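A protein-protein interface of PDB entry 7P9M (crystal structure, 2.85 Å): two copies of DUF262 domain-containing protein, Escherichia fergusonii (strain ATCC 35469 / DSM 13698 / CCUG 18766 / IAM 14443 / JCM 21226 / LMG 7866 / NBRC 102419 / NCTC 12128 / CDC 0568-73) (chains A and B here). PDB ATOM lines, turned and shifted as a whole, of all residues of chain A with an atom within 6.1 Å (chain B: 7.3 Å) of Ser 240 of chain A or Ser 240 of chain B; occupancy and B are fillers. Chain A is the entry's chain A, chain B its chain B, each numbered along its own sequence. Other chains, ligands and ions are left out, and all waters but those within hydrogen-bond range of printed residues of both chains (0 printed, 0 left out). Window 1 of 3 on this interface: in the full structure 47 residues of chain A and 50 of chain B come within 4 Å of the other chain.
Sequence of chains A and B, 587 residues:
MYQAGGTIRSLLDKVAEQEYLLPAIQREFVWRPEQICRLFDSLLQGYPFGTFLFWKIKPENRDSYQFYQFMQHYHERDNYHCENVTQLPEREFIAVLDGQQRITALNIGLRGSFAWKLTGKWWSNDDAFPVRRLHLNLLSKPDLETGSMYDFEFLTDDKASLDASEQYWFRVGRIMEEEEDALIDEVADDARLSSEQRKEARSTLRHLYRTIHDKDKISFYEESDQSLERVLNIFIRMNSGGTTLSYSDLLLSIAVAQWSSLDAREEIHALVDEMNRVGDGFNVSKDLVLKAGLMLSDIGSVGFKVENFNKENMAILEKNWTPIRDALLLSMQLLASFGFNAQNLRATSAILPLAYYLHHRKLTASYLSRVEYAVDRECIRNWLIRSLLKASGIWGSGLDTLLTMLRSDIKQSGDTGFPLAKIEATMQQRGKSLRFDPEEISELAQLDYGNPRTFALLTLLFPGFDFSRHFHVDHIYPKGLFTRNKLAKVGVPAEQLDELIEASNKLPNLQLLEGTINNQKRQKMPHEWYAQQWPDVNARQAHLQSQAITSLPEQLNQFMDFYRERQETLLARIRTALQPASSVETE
Of the 15 printed residues of chain A, 11 touch a printed residue of chain B. Among the printed residues, 23 pairs touch across the chains.
Of the printed residues of chain B, Asp 98 of chain A touches Ser 240 (2.7 Å). Of the printed residues of chain B, Met 238 of chain A touches Gly 50 (2.8 Å) and Arg 102 (2.9 Å). Printed residues of chain B within 4 Å of Ser 240 of chain A: Arg 102 (3.996 Å), Ser 240 (3.97 Å) and Thr 243 (3.0 Å). Printed residues of chain B within 4 Å of Gly 241 of chain A: Thr 243 (3.7 Å). Gly 242 of chain A touches none of the printed residues of chain B. Printed residues of chain A within 4 Å of Arg 102 of chain B: Arg 237 (3.4 Å), Met 238 (2.9 Å), Asn 239 (3.3 Å) and Ser 240 (3.996 Å). Of the printed residues of chain A, Ile 236 of chain B touches Thr 244 (3.8 Å). Of the printed residues of chain A, Ser 240 of chain B touches Asp 98 (2.7 Å), Arg 102 (3.4 Å), Ser 240 (3.97 Å) and Thr 244 (3.4 Å). Gly 241 of chain B touches none of the printed residues of chain A.
The side-chain amide nitrogen (ND2) of Asn 239 of chain A sits at hydrogen-bond distance from the backbone carbonyl oxygen (O) of Phe 235 of chain A, 3.0 Å away. OD1 of Asp 98 of chain A is in salt-bridge range of NH2 of Arg 102 of chain A, 3.1 Å away. The side-chain carboxylate (OD2) of Asp 98 of chain B lies within salt-bridge range of the guanidinium group (NH2) of Arg 102 of chain B, 3.2 Å away.
Gly 50 of chain A touches Asn 239 of chain B, and with the chains exchanged Asn 239 of chain A touches Gly 50 of chain B. Arg 102 of chain A touches Ser 240 of chain B, and with the chains exchanged Ser 240 of chain A touches Arg 102 of chain B. Thr 243 of chain A touches Gly 242 of chain B, but with the chains exchanged Gly 242 of chain A does not touch Thr 243 of chain B (4.4 Å). Thr 244 of chain A touches Ser 240 of chain B, but with the chains exchanged Ser 240 of chain A does not touch Thr 244 of chain B (6.2 Å). Of the 23 pairs that touch across the chains among the printed residues, 16 have their exchanged pair printed and touching as well.
The backbone carbonyl oxygen (O) of Met 238 of chain B is in hydrogen-bond range of the backbone NH (N) of Gly 50 of chain A. NH2 of Arg 102 of chain A sits at hydrogen-bond distance from OG of Ser 240 of chain B (3.4 Å). The backbone carbonyl oxygen of Met 238 of chain A is in hydrogen-bond range of the guanidinium group of Arg 102 of chain B, 2.9 Å away. OD1 of Asp 98 of chain A is in hydrogen-bond range of OG of Ser 240 of chain B, 2.7 Å away. The guanidinium group (NH1) of Arg 102 of chain B lies close to the backbone carbonyl oxygen (O) of Asn 239 of chain A, 3.4 Å away. OG1 of Thr 243 of chain B lies close to N of Thr 243 of chain A (3.2 Å). The backbone NH of Gly 50 of chain B sits at hydrogen-bond distance from the backbone carbonyl oxygen of Met 238 of chain A, at 2.8 Å.
Gly 50 of chain A touches Asn 239 of chain B (CA to ND2, 3.95 Å). Arg 102 of chain A touches Arg 237 of chain B. Met 238 of chain B touches Arg 102 of chain A. Asn 239 of chain B touches Arg 102 of chain A (C to NH1, 3.8 Å). Thr 244 of chain B touches Ile 236 of chain A (OG1 to CD1, 3.7 Å). Arg 102 of chain B touches Arg 237 of chain A (CD to O, 3.4 Å). Ser 240 of chain A touches Arg 102 of chain B (CA to NH2, 3.996 Å). OG of Ser 240 of chain A touches CG2 of Thr 243 of chain B (3.0 Å). OG1 of Thr 243 of chain A touches N of Gly 242 of chain B, 3.6 Å away. Thr 244 of chain A touches Ile 236 of chain B.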
ATOM      1  N   GLY A  50     -21.552   9.342  -0.071  1.00  0.00           N
ATOM      2  CA  GLY A  50     -20.263   9.719  -0.643  1.00  0.00           C
ATOM      3  C   GLY A  50     -19.826   8.665  -1.611  1.00  0.00           C
ATOM      4  O   GLY A  50     -20.450   7.612  -1.664  1.00  0.00           O
ATOM      5  N   THR A  51     -18.754   8.933  -2.327  1.00  0.00           N
ATOM      6  CA  THR A  51     -18.261   7.972  -3.324  1.00  0.00           C
ATOM      7  C   THR A  51     -17.659   6.793  -2.576  1.00  0.00           C
ATOM      8  O   THR A  51     -17.055   7.023  -1.531  1.00  0.00           O
ATOM      9  CB  THR A  51     -17.325   8.682  -4.298  1.00  0.00           C
ATOM     10  OG1 THR A  51     -17.919   9.929  -4.654  1.00  0.00           O
ATOM     11  CG2 THR A  51     -17.078   7.862  -5.537  1.00  0.00           C
ATOM     12  N   ASP A  98     -14.096   1.263   0.828  1.00  0.00           N
ATOM     13  CA  ASP A  98     -14.766   2.423   1.454  1.00  0.00           C
ATOM     14  C   ASP A  98     -16.261   2.217   1.353  1.00  0.00           C
ATOM     15  O   ASP A  98     -16.707   1.846   0.283  1.00  0.00           O
ATOM     16  CB  ASP A  98     -14.408   3.716   0.741  1.00  0.00           C
ATOM     17  CG  ASP A  98     -15.049   4.941   1.356  1.00  0.00           C
ATOM     18  OD1 ASP A  98     -14.713   5.254   2.507  1.00  0.00           O
ATOM     19  OD2 ASP A  98     -15.877   5.568   0.676  1.00  0.00           O
ATOM     20  N   GLY A  99     -16.981   2.469   2.435  1.00  0.00           N
ATOM     21  CA  GLY A  99     -18.442   2.309   2.431  1.00  0.00           C
ATOM     22  C   GLY A  99     -18.804   1.022   3.103  1.00  0.00           C
ATOM     23  O   GLY A  99     -19.963   0.632   3.041  1.00  0.00           O
ATOM     24  N   ARG A 102     -21.561   1.688   5.484  1.00  0.00           N
ATOM     25  CA  ARG A 102     -22.795   2.267   4.900  1.00  0.00           C
ATOM     26  C   ARG A 102     -23.601   1.179   4.203  1.00  0.00           C
ATOM     27  O   ARG A 102     -24.810   1.116   4.407  1.00  0.00           O
ATOM     28  CB  ARG A 102     -22.411   3.419   3.980  1.00  0.00           C
ATOM     29  CG  ARG A 102     -21.955   4.666   4.712  1.00  0.00           C
ATOM     30  CD  ARG A 102     -20.972   5.417   3.847  1.00  0.00           C
ATOM     31  NE  ARG A 102     -19.614   5.094   4.237  1.00  0.00           N
ATOM     32  CZ  ARG A 102     -18.539   5.597   3.657  1.00  0.00           C
ATOM     33  NH1 ARG A 102     -18.664   6.450   2.655  1.00  0.00           N
ATOM     34  NH2 ARG A 102     -17.341   5.234   4.075  1.00  0.00           N
ATOM     35  N   PHE A 235      -8.572   9.696  -5.054  1.00  0.00           N
ATOM     36  CA  PHE A 235      -9.858   9.799  -4.338  1.00  0.00           C
ATOM     37  C   PHE A 235      -9.642  10.677  -3.119  1.00  0.00           C
ATOM     38  O   PHE A 235     -10.445  11.562  -2.865  1.00  0.00           O
ATOM     39  CB  PHE A 235     -10.320   8.388  -3.970  1.00  0.00           C
ATOM     40  CG  PHE A 235     -11.456   8.238  -2.993  1.00  0.00           C
ATOM     41  CD1 PHE A 235     -12.770   8.307  -3.418  1.00  0.00           C
ATOM     42  CD2 PHE A 235     -11.216   7.944  -1.663  1.00  0.00           C
ATOM     43  CE1 PHE A 235     -13.815   8.142  -2.526  1.00  0.00           C
ATOM     44  CE2 PHE A 235     -12.263   7.779  -0.771  1.00  0.00           C
ATOM     45  CZ  PHE A 235     -13.561   7.877  -1.205  1.00  0.00           C
ATOM     46  N   ILE A 236      -8.559  10.445  -2.391  1.00  0.00           N
ATOM     47  CA  ILE A 236      -8.370  11.160  -1.097  1.00  0.00           C
ATOM     48  C   ILE A 236      -8.114  12.640  -1.357  1.00  0.00           C
ATOM     49  O   ILE A 236      -8.488  13.462  -0.511  1.00  0.00           O
ATOM     50  CB  ILE A 236      -7.256  10.484  -0.282  1.00  0.00           C
ATOM     51  CG1 ILE A 236      -7.321   8.963  -0.401  1.00  0.00           C
ATOM     52  CG2 ILE A 236      -7.290  10.915   1.171  1.00  0.00           C
ATOM     53  CD1 ILE A 236      -6.074   8.269   0.077  1.00  0.00           C
ATOM     54  N   ARG A 237      -7.502  12.960  -2.493  1.00  0.00           N
ATOM     55  CA  ARG A 237      -7.284  14.383  -2.841  1.00  0.00           C
ATOM     56  C   ARG A 237      -8.644  15.044  -2.998  1.00  0.00           C
ATOM     57  O   ARG A 237      -8.845  16.104  -2.423  1.00  0.00           O
ATOM     58  CB  ARG A 237      -6.525  14.497  -4.162  1.00  0.00           C
ATOM     59  CG  ARG A 237      -5.389  15.504  -4.142  1.00  0.00           C
ATOM     60  CD  ARG A 237      -4.520  15.351  -5.369  1.00  0.00           C
ATOM     61  NE  ARG A 237      -3.376  14.492  -5.116  1.00  0.00           N
ATOM     62  CZ  ARG A 237      -2.985  13.527  -5.933  1.00  0.00           C
ATOM     63  NH1 ARG A 237      -3.644  13.308  -7.057  1.00  0.00           N
ATOM     64  NH2 ARG A 237      -1.934  12.789  -5.626  1.00  0.00           N
ATOM     65  N   MET A 238      -9.496  14.460  -3.830  1.00  0.00           N
ATOM     66  CA  MET A 238     -10.778  15.103  -4.185  1.00  0.00           C
ATOM     67  C   MET A 238     -11.811  14.949  -3.082  1.00  0.00           C
ATOM     68  O   MET A 238     -12.769  15.712  -3.077  1.00  0.00           O
ATOM     69  CB  MET A 238     -11.311  14.454  -5.457  1.00  0.00           C
ATOM     70  CG  MET A 238     -10.301  14.364  -6.580  1.00  0.00           C
ATOM     71  SD  MET A 238      -9.357  15.878  -6.823  1.00  0.00           S
ATOM     72  CE  MET A 238     -10.316  16.677  -8.105  1.00  0.00           C
ATOM     73  N   ASN A 239     -11.659  13.957  -2.226  1.00  0.00           N
ATOM     74  CA  ASN A 239     -12.706  13.725  -1.210  1.00  0.00           C
ATOM     75  C   ASN A 239     -12.094  14.005   0.152  1.00  0.00           C
ATOM     76  O   ASN A 239     -11.081  14.701   0.214  1.00  0.00           O
ATOM     77  CB  ASN A 239     -13.281  12.316  -1.297  1.00  0.00           C
ATOM     78  CG  ASN A 239     -14.067  12.038  -2.558  1.00  0.00           C
ATOM     79  OD1 ASN A 239     -15.293  12.007  -2.534  1.00  0.00           O
ATOM     80  ND2 ASN A 239     -13.372  11.796  -3.655  1.00  0.00           N
ATOM     81  N   SER A 240     -12.689  13.470   1.211  1.00  0.00           N
ATOM     82  CA  SER A 240     -12.201  13.714   2.592  1.00  0.00           C
ATOM     83  C   SER A 240     -10.819  13.115   2.791  1.00  0.00           C
ATOM     84  O   SER A 240     -10.663  11.909   2.573  1.00  0.00           O
ATOM     85  CB  SER A 240     -13.132  13.115   3.584  1.00  0.00           C
ATOM     86  OG  SER A 240     -13.170  11.701   3.450  1.00  0.00           O
ATOM     87  N   GLY A 241      -9.854  13.942   3.177  1.00  0.00           N
ATOM     88  CA  GLY A 241      -8.487  13.452   3.422  1.00  0.00           C
ATOM     89  C   GLY A 241      -8.111  13.735   4.847  1.00  0.00           C
ATOM     90  O   GLY A 241      -7.346  12.958   5.438  1.00  0.00           O
ATOM     91  N   GLY A 242      -8.684  14.796   5.394  1.00  0.00           N
ATOM     92  CA  GLY A 242      -8.440  15.104   6.804  1.00  0.00           C
ATOM     93  C   GLY A 242      -9.421  14.340   7.649  1.00  0.00           C
ATOM     94  O   GLY A 242      -9.769  14.850   8.718  1.00  0.00           O
ATOM     95  N   THR A 243      -9.844  13.167   7.177  1.00  0.00           N
ATOM     96  CA  THR A 243     -10.813  12.334   7.922  1.00  0.00           C
ATOM     97  C   THR A 243     -11.928  13.247   8.417  1.00  0.00           C
ATOM     98  O   THR A 243     -12.155  13.310   9.639  1.00  0.00           O
ATOM     99  CB  THR A 243     -10.101  11.486   8.985  1.00  0.00           C
ATOM    100  OG1 THR A 243     -10.995  10.532   9.563  1.00  0.00           O
ATOM    101  CG2 THR A 243      -9.507  12.312  10.106  1.00  0.00           C
ATOM    102  N   THR A 244     -12.611  13.904   7.487  1.00  0.00           N
ATOM    103  CA  THR A 244     -13.670  14.877   7.846  1.00  0.00           C
ATOM    104  C   THR A 244     -13.170  15.733   8.991  1.00  0.00           C
ATOM    105  O   THR A 244     -12.163  16.429   8.814  1.00  0.00           O
ATOM    106  CB  THR A 244     -15.010  14.214   8.180  1.00  0.00           C
ATOM    107  OG1 THR A 244     -14.875  13.223   9.198  1.00  0.00           O
ATOM    108  CG2 THR A 244     -15.665  13.595   6.966  1.00  0.00           C
ATOM    109  N   GLY B  50     -15.381  15.977  -4.088  1.00  0.00           N
ATOM    110  CA  GLY B  50     -16.406  15.482  -3.165  1.00  0.00           C
ATOM    111  C   GLY B  50     -17.177  16.618  -2.557  1.00  0.00           C
ATOM    112  O   GLY B  50     -16.861  17.770  -2.845  1.00  0.00           O
ATOM    113  N   THR B  51     -18.107  16.306  -1.672  1.00  0.00           N
ATOM    114  CA  THR B  51     -18.945  17.350  -1.047  1.00  0.00           C
ATOM    115  C   THR B  51     -18.135  18.071   0.030  1.00  0.00           C
ATOM    116  O   THR B  51     -17.299  17.423   0.657  1.00  0.00           O
ATOM    117  CB  THR B  51     -20.268  16.715  -0.625  1.00  0.00           C
ATOM    118  OG1 THR B  51     -20.875  16.229  -1.821  1.00  0.00           O
ATOM    119  CG2 THR B  51     -21.212  17.681   0.049  1.00  0.00           C
ATOM    120  N   ASP B  98     -14.728  21.578   6.158  1.00  0.00           N
ATOM    121  CA  ASP B  98     -14.088  20.475   5.393  1.00  0.00           C
ATOM    122  C   ASP B  98     -13.790  20.943   3.975  1.00  0.00           C
ATOM    123  O   ASP B  98     -14.649  21.608   3.397  1.00  0.00           O
ATOM    124  CB  ASP B  98     -14.974  19.243   5.266  1.00  0.00           C
ATOM    125  CG  ASP B  98     -14.180  17.982   4.978  1.00  0.00           C
ATOM    126  OD1 ASP B  98     -13.083  17.844   5.545  1.00  0.00           O
ATOM    127  OD2 ASP B  98     -14.654  17.158   4.182  1.00  0.00           O
ATOM    128  N   GLY B  99     -12.627  20.567   3.446  1.00  0.00           N
ATOM    129  CA  GLY B  99     -12.242  20.971   2.086  1.00  0.00           C
ATOM    130  C   GLY B  99     -11.302  22.140   2.119  1.00  0.00           C
ATOM    131  O   GLY B  99     -10.989  22.647   1.070  1.00  0.00           O
ATOM    132  N   ARG B 102      -8.405  21.751  -0.163  1.00  0.00           N
ATOM    133  CA  ARG B 102      -8.808  21.726  -1.578  1.00  0.00           C
ATOM    134  C   ARG B 102      -9.015  23.168  -2.025  1.00  0.00           C
ATOM    135  O   ARG B 102      -8.515  23.535  -3.078  1.00  0.00           O
ATOM    136  CB  ARG B 102     -10.053  20.858  -1.719  1.00  0.00           C
ATOM    137  CG  ARG B 102      -9.794  19.364  -1.588  1.00  0.00           C
ATOM    138  CD  ARG B 102     -11.066  18.549  -1.464  1.00  0.00           C
ATOM    139  NE  ARG B 102     -11.470  18.334  -0.085  1.00  0.00           N
ATOM    140  CZ  ARG B 102     -12.552  17.663   0.285  1.00  0.00           C
ATOM    141  NH1 ARG B 102     -13.347  17.129  -0.623  1.00  0.00           N
ATOM    142  NH2 ARG B 102     -12.838  17.522   1.563  1.00  0.00           N
ATOM    143  N   PHE B 235     -22.890  14.224   7.722  1.00  0.00           N
ATOM    144  CA  PHE B 235     -21.789  14.205   6.735  1.00  0.00           C
ATOM    145  C   PHE B 235     -20.872  13.042   7.067  1.00  0.00           C
ATOM    146  O   PHE B 235     -20.432  12.347   6.163  1.00  0.00           O
ATOM    147  CB  PHE B 235     -21.036  15.529   6.834  1.00  0.00           C
ATOM    148  CG  PHE B 235     -20.077  15.868   5.723  1.00  0.00           C
ATOM    149  CD1 PHE B 235     -20.538  16.270   4.483  1.00  0.00           C
ATOM    150  CD2 PHE B 235     -18.712  15.835   5.939  1.00  0.00           C
ATOM    151  CE1 PHE B 235     -19.653  16.601   3.473  1.00  0.00           C
ATOM    152  CE2 PHE B 235     -17.828  16.166   4.926  1.00  0.00           C
ATOM    153  CZ  PHE B 235     -18.300  16.549   3.696  1.00  0.00           C
ATOM    154  N   ILE B 236     -20.630  12.811   8.345  1.00  0.00           N
ATOM    155  CA  ILE B 236     -19.643  11.756   8.690  1.00  0.00           C
ATOM    156  C   ILE B 236     -20.265  10.386   8.417  1.00  0.00           C
ATOM    157  O   ILE B 236     -19.526   9.468   8.063  1.00  0.00           O
ATOM    158  CB  ILE B 236     -19.139  11.954  10.129  1.00  0.00           C
ATOM    159  CG1 ILE B 236     -18.474  13.320  10.299  1.00  0.00           C
ATOM    160  CG2 ILE B 236     -18.196  10.841  10.557  1.00  0.00           C
ATOM    161  CD1 ILE B 236     -17.778  13.497  11.625  1.00  0.00           C
ATOM    162  N   ARG B 237     -21.577  10.245   8.553  1.00  0.00           N
ATOM    163  CA  ARG B 237     -22.179   8.936   8.212  1.00  0.00           C
ATOM    164  C   ARG B 237     -22.234   8.801   6.697  1.00  0.00           C
ATOM    165  O   ARG B 237     -21.726   7.803   6.184  1.00  0.00           O
ATOM    166  CB  ARG B 237     -23.565   8.792   8.838  1.00  0.00           C
ATOM    167  CG  ARG B 237     -23.545   8.714  10.356  1.00  0.00           C
ATOM    168  CD  ARG B 237     -24.937   8.620  10.947  1.00  0.00           C
ATOM    169  NE  ARG B 237     -24.902   8.522  12.396  1.00  0.00           N
ATOM    170  CZ  ARG B 237     -24.792   9.564  13.209  1.00  0.00           C
ATOM    171  NH1 ARG B 237     -24.707  10.784  12.712  1.00  0.00           N
ATOM    172  NH2 ARG B 237     -24.770   9.380  14.516  1.00  0.00           N
ATOM    173  N   MET B 238     -22.889   9.744   6.029  1.00  0.00           N
ATOM    174  CA  MET B 238     -23.081   9.659   4.565  1.00  0.00           C
ATOM    175  C   MET B 238     -21.729   9.668   3.864  1.00  0.00           C
ATOM    176  O   MET B 238     -21.444   8.705   3.148  1.00  0.00           O
ATOM    177  CB  MET B 238     -23.916  10.841   4.087  1.00  0.00           C
ATOM    178  CG  MET B 238     -25.303  10.901   4.684  1.00  0.00           C
ATOM    179  SD  MET B 238     -26.108   9.296   4.762  1.00  0.00           S
ATOM    180  CE  MET B 238     -27.019   9.306   3.220  1.00  0.00           C
ATOM    181  N   ASN B 239     -20.920  10.704   4.071  1.00  0.00           N
ATOM    182  CA  ASN B 239     -19.554  10.711   3.486  1.00  0.00           C
ATOM    183  C   ASN B 239     -18.668   9.809   4.345  1.00  0.00           C
ATOM    184  O   ASN B 239     -19.169   9.260   5.316  1.00  0.00           O
ATOM    185  CB  ASN B 239     -19.066  12.126   3.202  1.00  0.00           C
ATOM    186  CG  ASN B 239     -19.966  12.882   2.248  1.00  0.00           C
ATOM    187  OD1 ASN B 239     -21.110  13.189   2.569  1.00  0.00           O
ATOM    188  ND2 ASN B 239     -19.457  13.191   1.069  1.00  0.00           N
ATOM    189  N   SER B 240     -17.387   9.665   4.032  1.00  0.00           N
ATOM    190  CA  SER B 240     -16.555   8.664   4.754  1.00  0.00           C
ATOM    191  C   SER B 240     -16.269   9.045   6.204  1.00  0.00           C
ATOM    192  O   SER B 240     -16.217  10.243   6.495  1.00  0.00           O
ATOM    193  CB  SER B 240     -15.288   8.386   4.010  1.00  0.00           C
ATOM    194  OG  SER B 240     -15.568   7.770   2.764  1.00  0.00           O
ATOM    195  N   GLY B 241     -15.984   8.038   7.028  1.00  0.00           N
ATOM    196  CA  GLY B 241     -15.534   8.274   8.410  1.00  0.00           C
ATOM    197  C   GLY B 241     -14.310   7.403   8.617  1.00  0.00           C
ATOM    198  O   GLY B 241     -14.240   6.360   7.960  1.00  0.00           O
ATOM    199  N   GLY B 242     -13.327   7.848   9.401  1.00  0.00           N
ATOM    200  CA  GLY B 242     -12.074   7.075   9.509  1.00  0.00           C
ATOM    201  C   GLY B 242     -11.494   6.920   8.128  1.00  0.00           C
ATOM    202  O   GLY B 242     -11.442   5.787   7.635  1.00  0.00           O
ATOM    203  N   THR B 243     -11.076   8.041   7.528  1.00  0.00           N
ATOM    204  CA  THR B 243     -10.557   8.040   6.134  1.00  0.00           C
ATOM    205  C   THR B 243      -9.366   7.090   5.988  1.00  0.00           C
ATOM    206  O   THR B 243      -8.487   7.105   6.877  1.00  0.00           O
ATOM    207  CB  THR B 243     -10.290   9.474   5.655  1.00  0.00           C
ATOM    208  OG1 THR B 243      -9.339  10.059   6.545  1.00  0.00           O
ATOM    209  CG2 THR B 243     -11.525  10.345   5.581  1.00  0.00           C
ATOM    210  N   THR B 244      -9.337   6.326   4.893  1.00  0.00           N
ATOM    211  CA  THR B 244      -8.239   5.376   4.621  1.00  0.00           C
ATOM    212  C   THR B 244      -6.934   6.113   4.795  1.00  0.00           C
ATOM    213  O   THR B 244      -6.793   7.179   4.194  1.00  0.00           O
ATOM    214  CB  THR B 244      -8.240   4.984   3.146  1.00  0.00           C
ATOM    215  OG1 THR B 244      -8.082   6.184   2.392  1.00  0.00           O
ATOM    216  CG2 THR B 244      -9.505   4.273   2.722  1.00  0.00           C
